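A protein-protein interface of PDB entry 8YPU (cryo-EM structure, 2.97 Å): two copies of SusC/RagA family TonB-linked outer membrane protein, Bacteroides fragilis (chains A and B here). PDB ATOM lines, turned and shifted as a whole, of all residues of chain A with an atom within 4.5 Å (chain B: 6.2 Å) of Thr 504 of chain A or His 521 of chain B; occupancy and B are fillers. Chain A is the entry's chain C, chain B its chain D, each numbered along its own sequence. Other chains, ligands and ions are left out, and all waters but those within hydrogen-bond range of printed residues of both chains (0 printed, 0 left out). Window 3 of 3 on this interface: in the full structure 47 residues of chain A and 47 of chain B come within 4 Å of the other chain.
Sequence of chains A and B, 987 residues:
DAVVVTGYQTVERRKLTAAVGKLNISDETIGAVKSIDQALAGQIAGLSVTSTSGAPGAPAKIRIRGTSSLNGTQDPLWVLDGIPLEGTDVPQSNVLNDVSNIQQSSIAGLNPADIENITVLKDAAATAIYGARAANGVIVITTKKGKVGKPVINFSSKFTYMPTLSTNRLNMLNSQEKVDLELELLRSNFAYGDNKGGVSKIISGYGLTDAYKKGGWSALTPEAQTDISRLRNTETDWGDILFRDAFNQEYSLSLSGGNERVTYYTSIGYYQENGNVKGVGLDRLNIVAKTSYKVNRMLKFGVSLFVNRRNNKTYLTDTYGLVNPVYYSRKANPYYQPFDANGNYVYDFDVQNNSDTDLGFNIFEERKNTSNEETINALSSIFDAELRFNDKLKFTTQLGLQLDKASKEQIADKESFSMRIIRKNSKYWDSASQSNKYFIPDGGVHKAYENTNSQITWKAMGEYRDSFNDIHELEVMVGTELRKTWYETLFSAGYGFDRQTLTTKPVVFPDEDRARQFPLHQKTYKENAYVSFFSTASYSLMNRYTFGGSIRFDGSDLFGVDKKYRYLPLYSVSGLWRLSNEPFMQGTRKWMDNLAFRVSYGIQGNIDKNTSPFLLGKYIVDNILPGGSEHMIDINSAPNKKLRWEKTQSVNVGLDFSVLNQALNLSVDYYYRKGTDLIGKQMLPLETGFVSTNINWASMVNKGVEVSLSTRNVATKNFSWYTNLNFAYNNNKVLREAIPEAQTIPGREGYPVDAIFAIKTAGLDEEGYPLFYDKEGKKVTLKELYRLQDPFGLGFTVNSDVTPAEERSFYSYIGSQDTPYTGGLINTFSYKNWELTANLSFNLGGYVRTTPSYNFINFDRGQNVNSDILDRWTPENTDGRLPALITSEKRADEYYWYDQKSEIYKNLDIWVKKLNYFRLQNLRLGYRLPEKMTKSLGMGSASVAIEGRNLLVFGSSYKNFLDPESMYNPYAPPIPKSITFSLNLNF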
ATOM      1  N   HIS A 446     -12.573  -1.684  16.207  1.00  0.00           N
ATOM      2  CA  HIS A 446     -12.005  -2.407  15.080  1.00  0.00           C
ATOM      3  C   HIS A 446     -12.951  -3.542  14.731  1.00  0.00           C
ATOM      4  O   HIS A 446     -13.199  -4.421  15.560  1.00  0.00           O
ATOM      5  CB  HIS A 446     -10.616  -2.939  15.420  1.00  0.00           C
ATOM      6  CG  HIS A 446     -10.057  -3.878  14.399  1.00  0.00           C
ATOM      7  ND1 HIS A 446     -10.040  -5.241  14.579  1.00  0.00           N
ATOM      8  CD2 HIS A 446      -9.485  -3.651  13.197  1.00  0.00           C
ATOM      9  CE1 HIS A 446      -9.489  -5.816  13.527  1.00  0.00           C
ATOM     10  NE2 HIS A 446      -9.144  -4.872  12.672  1.00  0.00           N
ATOM     11  N   ALA A 448     -13.778  -6.616  11.934  1.00  0.00           N
ATOM     12  CA  ALA A 448     -13.150  -7.485  10.953  1.00  0.00           C
ATOM     13  C   ALA A 448     -14.196  -8.421  10.370  1.00  0.00           C
ATOM     14  O   ALA A 448     -14.892  -9.114  11.115  1.00  0.00           O
ATOM     15  CB  ALA A 448     -12.016  -8.290  11.584  1.00  0.00           C
ATOM     16  N   SER A 492     -16.041 -10.101  13.611  1.00  0.00           N
ATOM     17  CA  SER A 492     -15.507  -9.897  14.950  1.00  0.00           C
ATOM     18  C   SER A 492     -15.345  -8.409  15.212  1.00  0.00           C
ATOM     19  O   SER A 492     -14.951  -7.660  14.323  1.00  0.00           O
ATOM     20  CB  SER A 492     -14.164 -10.602  15.119  1.00  0.00           C
ATOM     21  OG  SER A 492     -13.838 -10.750  16.487  1.00  0.00           O
ATOM     22  N   ALA A 493     -15.653  -7.976  16.430  1.00  0.00           N
ATOM     23  CA  ALA A 493     -15.563  -6.568  16.785  1.00  0.00           C
ATOM     24  C   ALA A 493     -14.815  -6.404  18.097  1.00  0.00           C
ATOM     25  O   ALA A 493     -14.954  -7.218  19.012  1.00  0.00           O
ATOM     26  CB  ALA A 493     -16.942  -5.924  16.897  1.00  0.00           C
ATOM     27  N   GLY A 494     -14.017  -5.346  18.178  1.00  0.00           N
ATOM     28  CA  GLY A 494     -13.291  -5.033  19.389  1.00  0.00           C
ATOM     29  C   GLY A 494     -13.369  -3.562  19.729  1.00  0.00           C
ATOM     30  O   GLY A 494     -12.982  -2.717  18.922  1.00  0.00           O
ATOM     31  N   TYR A 495     -13.869  -3.252  20.919  1.00  0.00           N
ATOM     32  CA  TYR A 495     -14.067  -1.886  21.373  1.00  0.00           C
ATOM     33  C   TYR A 495     -13.011  -1.528  22.408  1.00  0.00           C
ATOM     34  O   TYR A 495     -12.496  -2.395  23.116  1.00  0.00           O
ATOM     35  CB  TYR A 495     -15.467  -1.703  21.960  1.00  0.00           C
ATOM     36  CG  TYR A 495     -16.578  -1.962  20.975  1.00  0.00           C
ATOM     37  CD1 TYR A 495     -17.112  -3.229  20.819  1.00  0.00           C
ATOM     38  CD2 TYR A 495     -17.092  -0.940  20.201  1.00  0.00           C
ATOM     39  CE1 TYR A 495     -18.120  -3.465  19.925  1.00  0.00           C
ATOM     40  CE2 TYR A 495     -18.103  -1.169  19.306  1.00  0.00           C
ATOM     41  CZ  TYR A 495     -18.612  -2.432  19.168  1.00  0.00           C
ATOM     42  OH  TYR A 495     -19.622  -2.660  18.265  1.00  0.00           O
ATOM     43  N   GLY A 496     -12.700  -0.241  22.504  1.00  0.00           N
ATOM     44  CA  GLY A 496     -11.529   0.167  23.241  1.00  0.00           C
ATOM     45  C   GLY A 496     -10.256   0.064  22.443  1.00  0.00           C
ATOM     46  O   GLY A 496      -9.168   0.163  23.017  1.00  0.00           O
ATOM     47  N   PHE A 497     -10.369  -0.098  21.130  1.00  0.00           N
ATOM     48  CA  PHE A 497      -9.235  -0.387  20.268  1.00  0.00           C
ATOM     49  C   PHE A 497      -8.313   0.821  20.170  1.00  0.00           C
ATOM     50  O   PHE A 497      -8.759   1.930  19.867  1.00  0.00           O
ATOM     51  CB  PHE A 497      -9.749  -0.789  18.889  1.00  0.00           C
ATOM     52  CG  PHE A 497      -8.697  -1.322  17.969  1.00  0.00           C
ATOM     53  CD1 PHE A 497      -8.226  -2.608  18.116  1.00  0.00           C
ATOM     54  CD2 PHE A 497      -8.208  -0.550  16.931  1.00  0.00           C
ATOM     55  CE1 PHE A 497      -7.269  -3.102  17.266  1.00  0.00           C
ATOM     56  CE2 PHE A 497      -7.257  -1.045  16.079  1.00  0.00           C
ATOM     57  CZ  PHE A 497      -6.786  -2.319  16.247  1.00  0.00           C
ATOM     58  N   LEU A 502      -3.020  -1.741  19.172  1.00  0.00           N
ATOM     59  CA  LEU A 502      -3.798  -2.912  18.769  1.00  0.00           C
ATOM     60  C   LEU A 502      -4.419  -3.630  19.962  1.00  0.00           C
ATOM     61  O   LEU A 502      -4.713  -4.826  19.893  1.00  0.00           O
ATOM     62  CB  LEU A 502      -2.956  -3.886  17.937  1.00  0.00           C
ATOM     63  CG  LEU A 502      -2.362  -3.383  16.625  1.00  0.00           C
ATOM     64  CD1 LEU A 502      -1.910  -4.540  15.785  1.00  0.00           C
ATOM     65  CD2 LEU A 502      -3.357  -2.554  15.866  1.00  0.00           C
ATOM     66  N   THR A 503      -4.645  -2.911  21.054  1.00  0.00           N
ATOM     67  CA  THR A 503      -5.262  -3.498  22.232  1.00  0.00           C
ATOM     68  C   THR A 503      -6.767  -3.270  22.212  1.00  0.00           C
ATOM     69  O   THR A 503      -7.307  -2.580  21.351  1.00  0.00           O
ATOM     70  CB  THR A 503      -4.656  -2.931  23.515  1.00  0.00           C
ATOM     71  OG1 THR A 503      -4.511  -1.511  23.401  1.00  0.00           O
ATOM     72  CG2 THR A 503      -3.307  -3.556  23.784  1.00  0.00           C
ATOM     73  N   THR A 504      -7.446  -3.869  23.185  1.00  0.00           N
ATOM     74  CA  THR A 504      -8.897  -3.876  23.257  1.00  0.00           C
ATOM     75  C   THR A 504      -9.306  -3.777  24.720  1.00  0.00           C
ATOM     76  O   THR A 504      -8.496  -4.001  25.622  1.00  0.00           O
ATOM     77  CB  THR A 504      -9.476  -5.145  22.608  1.00  0.00           C
ATOM     78  OG1 THR A 504      -8.710  -5.486  21.450  1.00  0.00           O
ATOM     79  CG2 THR A 504     -10.900  -4.940  22.177  1.00  0.00           C
ATOM     80  N   LYS A 505     -10.563  -3.417  24.953  1.00  0.00           N
ATOM     81  CA  LYS A 505     -11.113  -3.292  26.292  1.00  0.00           C
ATOM     82  C   LYS A 505     -12.413  -4.070  26.401  1.00  0.00           C
ATOM     83  O   LYS A 505     -13.148  -4.201  25.418  1.00  0.00           O
ATOM     84  CB  LYS A 505     -11.358  -1.821  26.645  1.00  0.00           C
ATOM     85  CG  LYS A 505     -10.192  -1.164  27.336  1.00  0.00           C
ATOM     86  CD  LYS A 505     -10.532   0.238  27.766  1.00  0.00           C
ATOM     87  CE  LYS A 505      -9.949   1.247  26.808  1.00  0.00           C
ATOM     88  NZ  LYS A 505      -9.828   2.592  27.423  1.00  0.00           N
ATOM     89  N   LEU B 490      -5.436 -12.499  13.012  1.00  0.00           N
ATOM     90  CA  LEU B 490      -6.646 -12.102  13.716  1.00  0.00           C
ATOM     91  C   LEU B 490      -7.208 -13.310  14.444  1.00  0.00           C
ATOM     92  O   LEU B 490      -7.340 -14.384  13.857  1.00  0.00           O
ATOM     93  CB  LEU B 490      -7.689 -11.535  12.756  1.00  0.00           C
ATOM     94  CG  LEU B 490      -9.107 -11.411  13.307  1.00  0.00           C
ATOM     95  CD1 LEU B 490      -9.331 -10.046  13.931  1.00  0.00           C
ATOM     96  CD2 LEU B 490     -10.116 -11.681  12.215  1.00  0.00           C
ATOM     97  N   PHE B 491      -7.538 -13.135  15.716  1.00  0.00           N
ATOM     98  CA  PHE B 491      -8.142 -14.181  16.523  1.00  0.00           C
ATOM     99  C   PHE B 491      -9.437 -13.657  17.117  1.00  0.00           C
ATOM    100  O   PHE B 491      -9.486 -12.527  17.606  1.00  0.00           O
ATOM    101  CB  PHE B 491      -7.187 -14.637  17.629  1.00  0.00           C
ATOM    102  CG  PHE B 491      -7.855 -15.399  18.729  1.00  0.00           C
ATOM    103  CD1 PHE B 491      -8.203 -16.724  18.559  1.00  0.00           C
ATOM    104  CD2 PHE B 491      -8.136 -14.790  19.936  1.00  0.00           C
ATOM    105  CE1 PHE B 491      -8.814 -17.420  19.567  1.00  0.00           C
ATOM    106  CE2 PHE B 491      -8.751 -15.485  20.940  1.00  0.00           C
ATOM    107  CZ  PHE B 491      -9.092 -16.800  20.755  1.00  0.00           C
ATOM    108  N   SER B 492     -10.489 -14.472  17.058  1.00  0.00           N
ATOM    109  CA  SER B 492     -11.782 -14.129  17.634  1.00  0.00           C
ATOM    110  C   SER B 492     -12.342 -15.329  18.381  1.00  0.00           C
ATOM    111  O   SER B 492     -12.201 -16.463  17.930  1.00  0.00           O
ATOM    112  CB  SER B 492     -12.764 -13.686  16.554  1.00  0.00           C
ATOM    113  OG  SER B 492     -13.853 -12.982  17.116  1.00  0.00           O
ATOM    114  N   ALA B 493     -12.971 -15.086  19.526  1.00  0.00           N
ATOM    115  CA  ALA B 493     -13.522 -16.160  20.339  1.00  0.00           C
ATOM    116  C   ALA B 493     -14.949 -15.834  20.745  1.00  0.00           C
ATOM    117  O   ALA B 493     -15.281 -14.678  21.015  1.00  0.00           O
ATOM    118  CB  ALA B 493     -12.678 -16.413  21.586  1.00  0.00           C
ATOM    119  N   GLU B 512      -9.681  -6.510  33.930  1.00  0.00           N
ATOM    120  CA  GLU B 512      -8.987  -6.476  32.654  1.00  0.00           C
ATOM    121  C   GLU B 512      -7.890  -7.524  32.564  1.00  0.00           C
ATOM    122  O   GLU B 512      -7.416  -7.807  31.461  1.00  0.00           O
ATOM    123  CB  GLU B 512      -8.393  -5.089  32.417  1.00  0.00           C
ATOM    124  CG  GLU B 512      -9.398  -4.059  31.941  1.00  0.00           C
ATOM    125  CD  GLU B 512      -8.843  -3.153  30.862  1.00  0.00           C
ATOM    126  OE1 GLU B 512      -8.279  -3.673  29.877  1.00  0.00           O
ATOM    127  OE2 GLU B 512      -8.978  -1.920  30.997  1.00  0.00           O
ATOM    128  N   PRO B 519      -8.891 -14.122  25.783  1.00  0.00           N
ATOM    129  CA  PRO B 519      -9.019 -13.077  24.762  1.00  0.00           C
ATOM    130  C   PRO B 519     -10.204 -13.337  23.849  1.00  0.00           C
ATOM    131  O   PRO B 519     -10.500 -14.479  23.492  1.00  0.00           O
ATOM    132  CB  PRO B 519      -7.691 -13.156  24.007  1.00  0.00           C
ATOM    133  CG  PRO B 519      -7.156 -14.485  24.313  1.00  0.00           C
ATOM    134  CD  PRO B 519      -7.604 -14.824  25.681  1.00  0.00           C
ATOM    135  N   LEU B 520     -10.887 -12.264  23.473  1.00  0.00           N
ATOM    136  CA  LEU B 520     -12.088 -12.355  22.660  1.00  0.00           C
ATOM    137  C   LEU B 520     -11.866 -11.894  21.231  1.00  0.00           C
ATOM    138  O   LEU B 520     -12.543 -12.376  20.322  1.00  0.00           O
ATOM    139  CB  LEU B 520     -13.206 -11.514  23.286  1.00  0.00           C
ATOM    140  CG  LEU B 520     -14.051 -12.112  24.409  1.00  0.00           C
ATOM    141  CD1 LEU B 520     -15.403 -11.452  24.457  1.00  0.00           C
ATOM    142  CD2 LEU B 520     -14.203 -13.606  24.265  1.00  0.00           C
ATOM    143  N   HIS B 521     -10.949 -10.955  21.023  1.00  0.00           N
ATOM    144  CA  HIS B 521     -10.672 -10.416  19.698  1.00  0.00           C
ATOM    145  C   HIS B 521      -9.273  -9.864  19.901  1.00  0.00           C
ATOM    146  O   HIS B 521      -9.068  -9.035  20.790  1.00  0.00           O
ATOM    147  CB  HIS B 521     -11.745  -9.418  19.289  1.00  0.00           C
ATOM    148  CG  HIS B 521     -11.395  -8.591  18.094  1.00  0.00           C
ATOM    149  ND1 HIS B 521     -11.807  -8.914  16.821  1.00  0.00           N
ATOM    150  CD2 HIS B 521     -10.682  -7.447  17.978  1.00  0.00           C
ATOM    151  CE1 HIS B 521     -11.364  -8.006  15.973  1.00  0.00           C
ATOM    152  NE2 HIS B 521     -10.676  -7.107  16.649  1.00  0.00           N
ATOM    153  N   GLN B 522      -8.318 -10.324  19.105  1.00  0.00           N
ATOM    154  CA  GLN B 522      -7.005  -9.703  19.046  1.00  0.00           C
ATOM    155  C   GLN B 522      -6.490  -9.688  17.616  1.00  0.00           C
ATOM    156  O   GLN B 522      -6.831 -10.545  16.803  1.00  0.00           O
ATOM    157  CB  GLN B 522      -5.997 -10.394  19.975  1.00  0.00           C
ATOM    158  CG  GLN B 522      -6.045 -11.898  20.004  1.00  0.00           C
ATOM    159  CD  GLN B 522      -5.305 -12.460  21.198  1.00  0.00           C
ATOM    160  OE1 GLN B 522      -5.030 -11.746  22.157  1.00  0.00           O
ATOM    161  NE2 GLN B 522      -4.966 -13.742  21.140  1.00  0.00           N
ATOM    162  N   LYS B 523      -5.678  -8.682  17.320  1.00  0.00           N
ATOM    163  CA  LYS B 523      -5.130  -8.459  15.993  1.00  0.00           C
ATOM    164  C   LYS B 523      -3.643  -8.171  16.105  1.00  0.00           C
ATOM    165  O   LYS B 523      -3.218  -7.416  16.981  1.00  0.00           O
ATOM    166  CB  LYS B 523      -5.833  -7.294  15.294  1.00  0.00           C
ATOM    167  CG  LYS B 523      -5.006  -6.656  14.203  1.00  0.00           C
ATOM    168  CD  LYS B 523      -5.623  -5.385  13.682  1.00  0.00           C
ATOM    169  CE  LYS B 523      -4.735  -4.754  12.633  1.00  0.00           C
ATOM    170  NZ  LYS B 523      -5.425  -3.660  11.910  1.00  0.00           N
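Printed residues of chain B that touch a printed residue of chain A: Leu 490, Ser 492, Glu 512, His 521 and Lys 523. Hydrophobic or aromatic side chains of chain B that line the printed part of chain A: Leu 490 and His 521. Of the 12 printed residues of chain A, 8 touch a printed residue of chain B. Hydrophobic or aromatic side chains of chain A that line the printed part of chain B: His 446, Ala 448 and Leu 502. Among the printed residues, 10 pairs touch across the chains. Among the printed residues, no Asp or Glu carboxylate lies within 4 Å of a Lys or Arg side-chain nitrogen of the other chain.
Of the printed residues of chain B, His 446 of chain A touches His 521 (2.9 Å) and Lys 523 (3.7 Å). Printed residues of chain B within 4 Å of Ala 448 of chain A: Leu 490. Of the printed residues of chain B, Gly 494 of chain A touches His 521. Thr 504 of chain A touches one residue of chain B. Of the printed residues of chain B, Lys 505 of chain A touches Glu 512 (3.9 Å). Of the printed residues of chain A, Leu 490 of chain B touches Ala 448 (3.9 Å). Printed residues of chain A within 4 Å of His 521 of chain B: His 446 (2.9 Å), Ser 492 (2.8 Å), Ala 493 (3.9 Å), Gly 494 (3.8 Å) and Thr 504 (3.6 Å). The nearest residue of chain B that does not touch Thr 504 of chain A is Glu 512 of chain B (4.3 Å).
His 446 of chain A touches Lys 523 of chain B. CB of Ala 448 of chain A touches CD2 of Leu 490 of chain B, at 3.9 Å. Ala 493 of chain A touches His 521 of chain B (O to CB, 3.9 Å). Gly 494 of chain A touches His 521 of chain B (CA to CD2, 3.8 Å). O of Lys 523 of chain B touches CD1 of Leu 502 of chain A, at 3.4 Å. His 521 of chain B touches Thr 504 of chain A (O to OG1, 3.6 Å). Glu 512 of chain B touches Lys 505 of chain A (OE2 to CG, 3.9 Å).
The backbone carbonyl oxygen (O) of His 446 of chain A sits at hydrogen-bond distance from the backbone NH (N) of Gly 494 of chain A (2.9 Å). The backbone carbonyl oxygen (O) of Ser 492 of chain A is in hydrogen-bond range of the backbone NH (N) of Ala 448 of chain A (2.9 Å). The backbone NH (N) of Lys 505 of chain A sits at hydrogen-bond distance from the backbone carbonyl oxygen (O) of Tyr 495 of chain A, at 2.9 Å.
Ser 492 of chain B touches its own counterpart, Ser 492 of chain A. Of the 10 pairs that touch across the chains among the printed residues, 1 has its exchanged pair printed and touching as well.
A ring nitrogen (ND1) of His 446 of chain A lies within hydrogen-bond range of a ring nitrogen (NE2) of His 521 of chain B, at 2.9 Å. The side-chain hydroxyl (OG) of Ser 492 of chain A lies within hydrogen-bond range of a ring nitrogen (ND1) of His 521 of chain B, 2.8 Å away. OG of Ser 492 of chain B sits close to OG of Ser 492 of chain A (2.3 Å).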
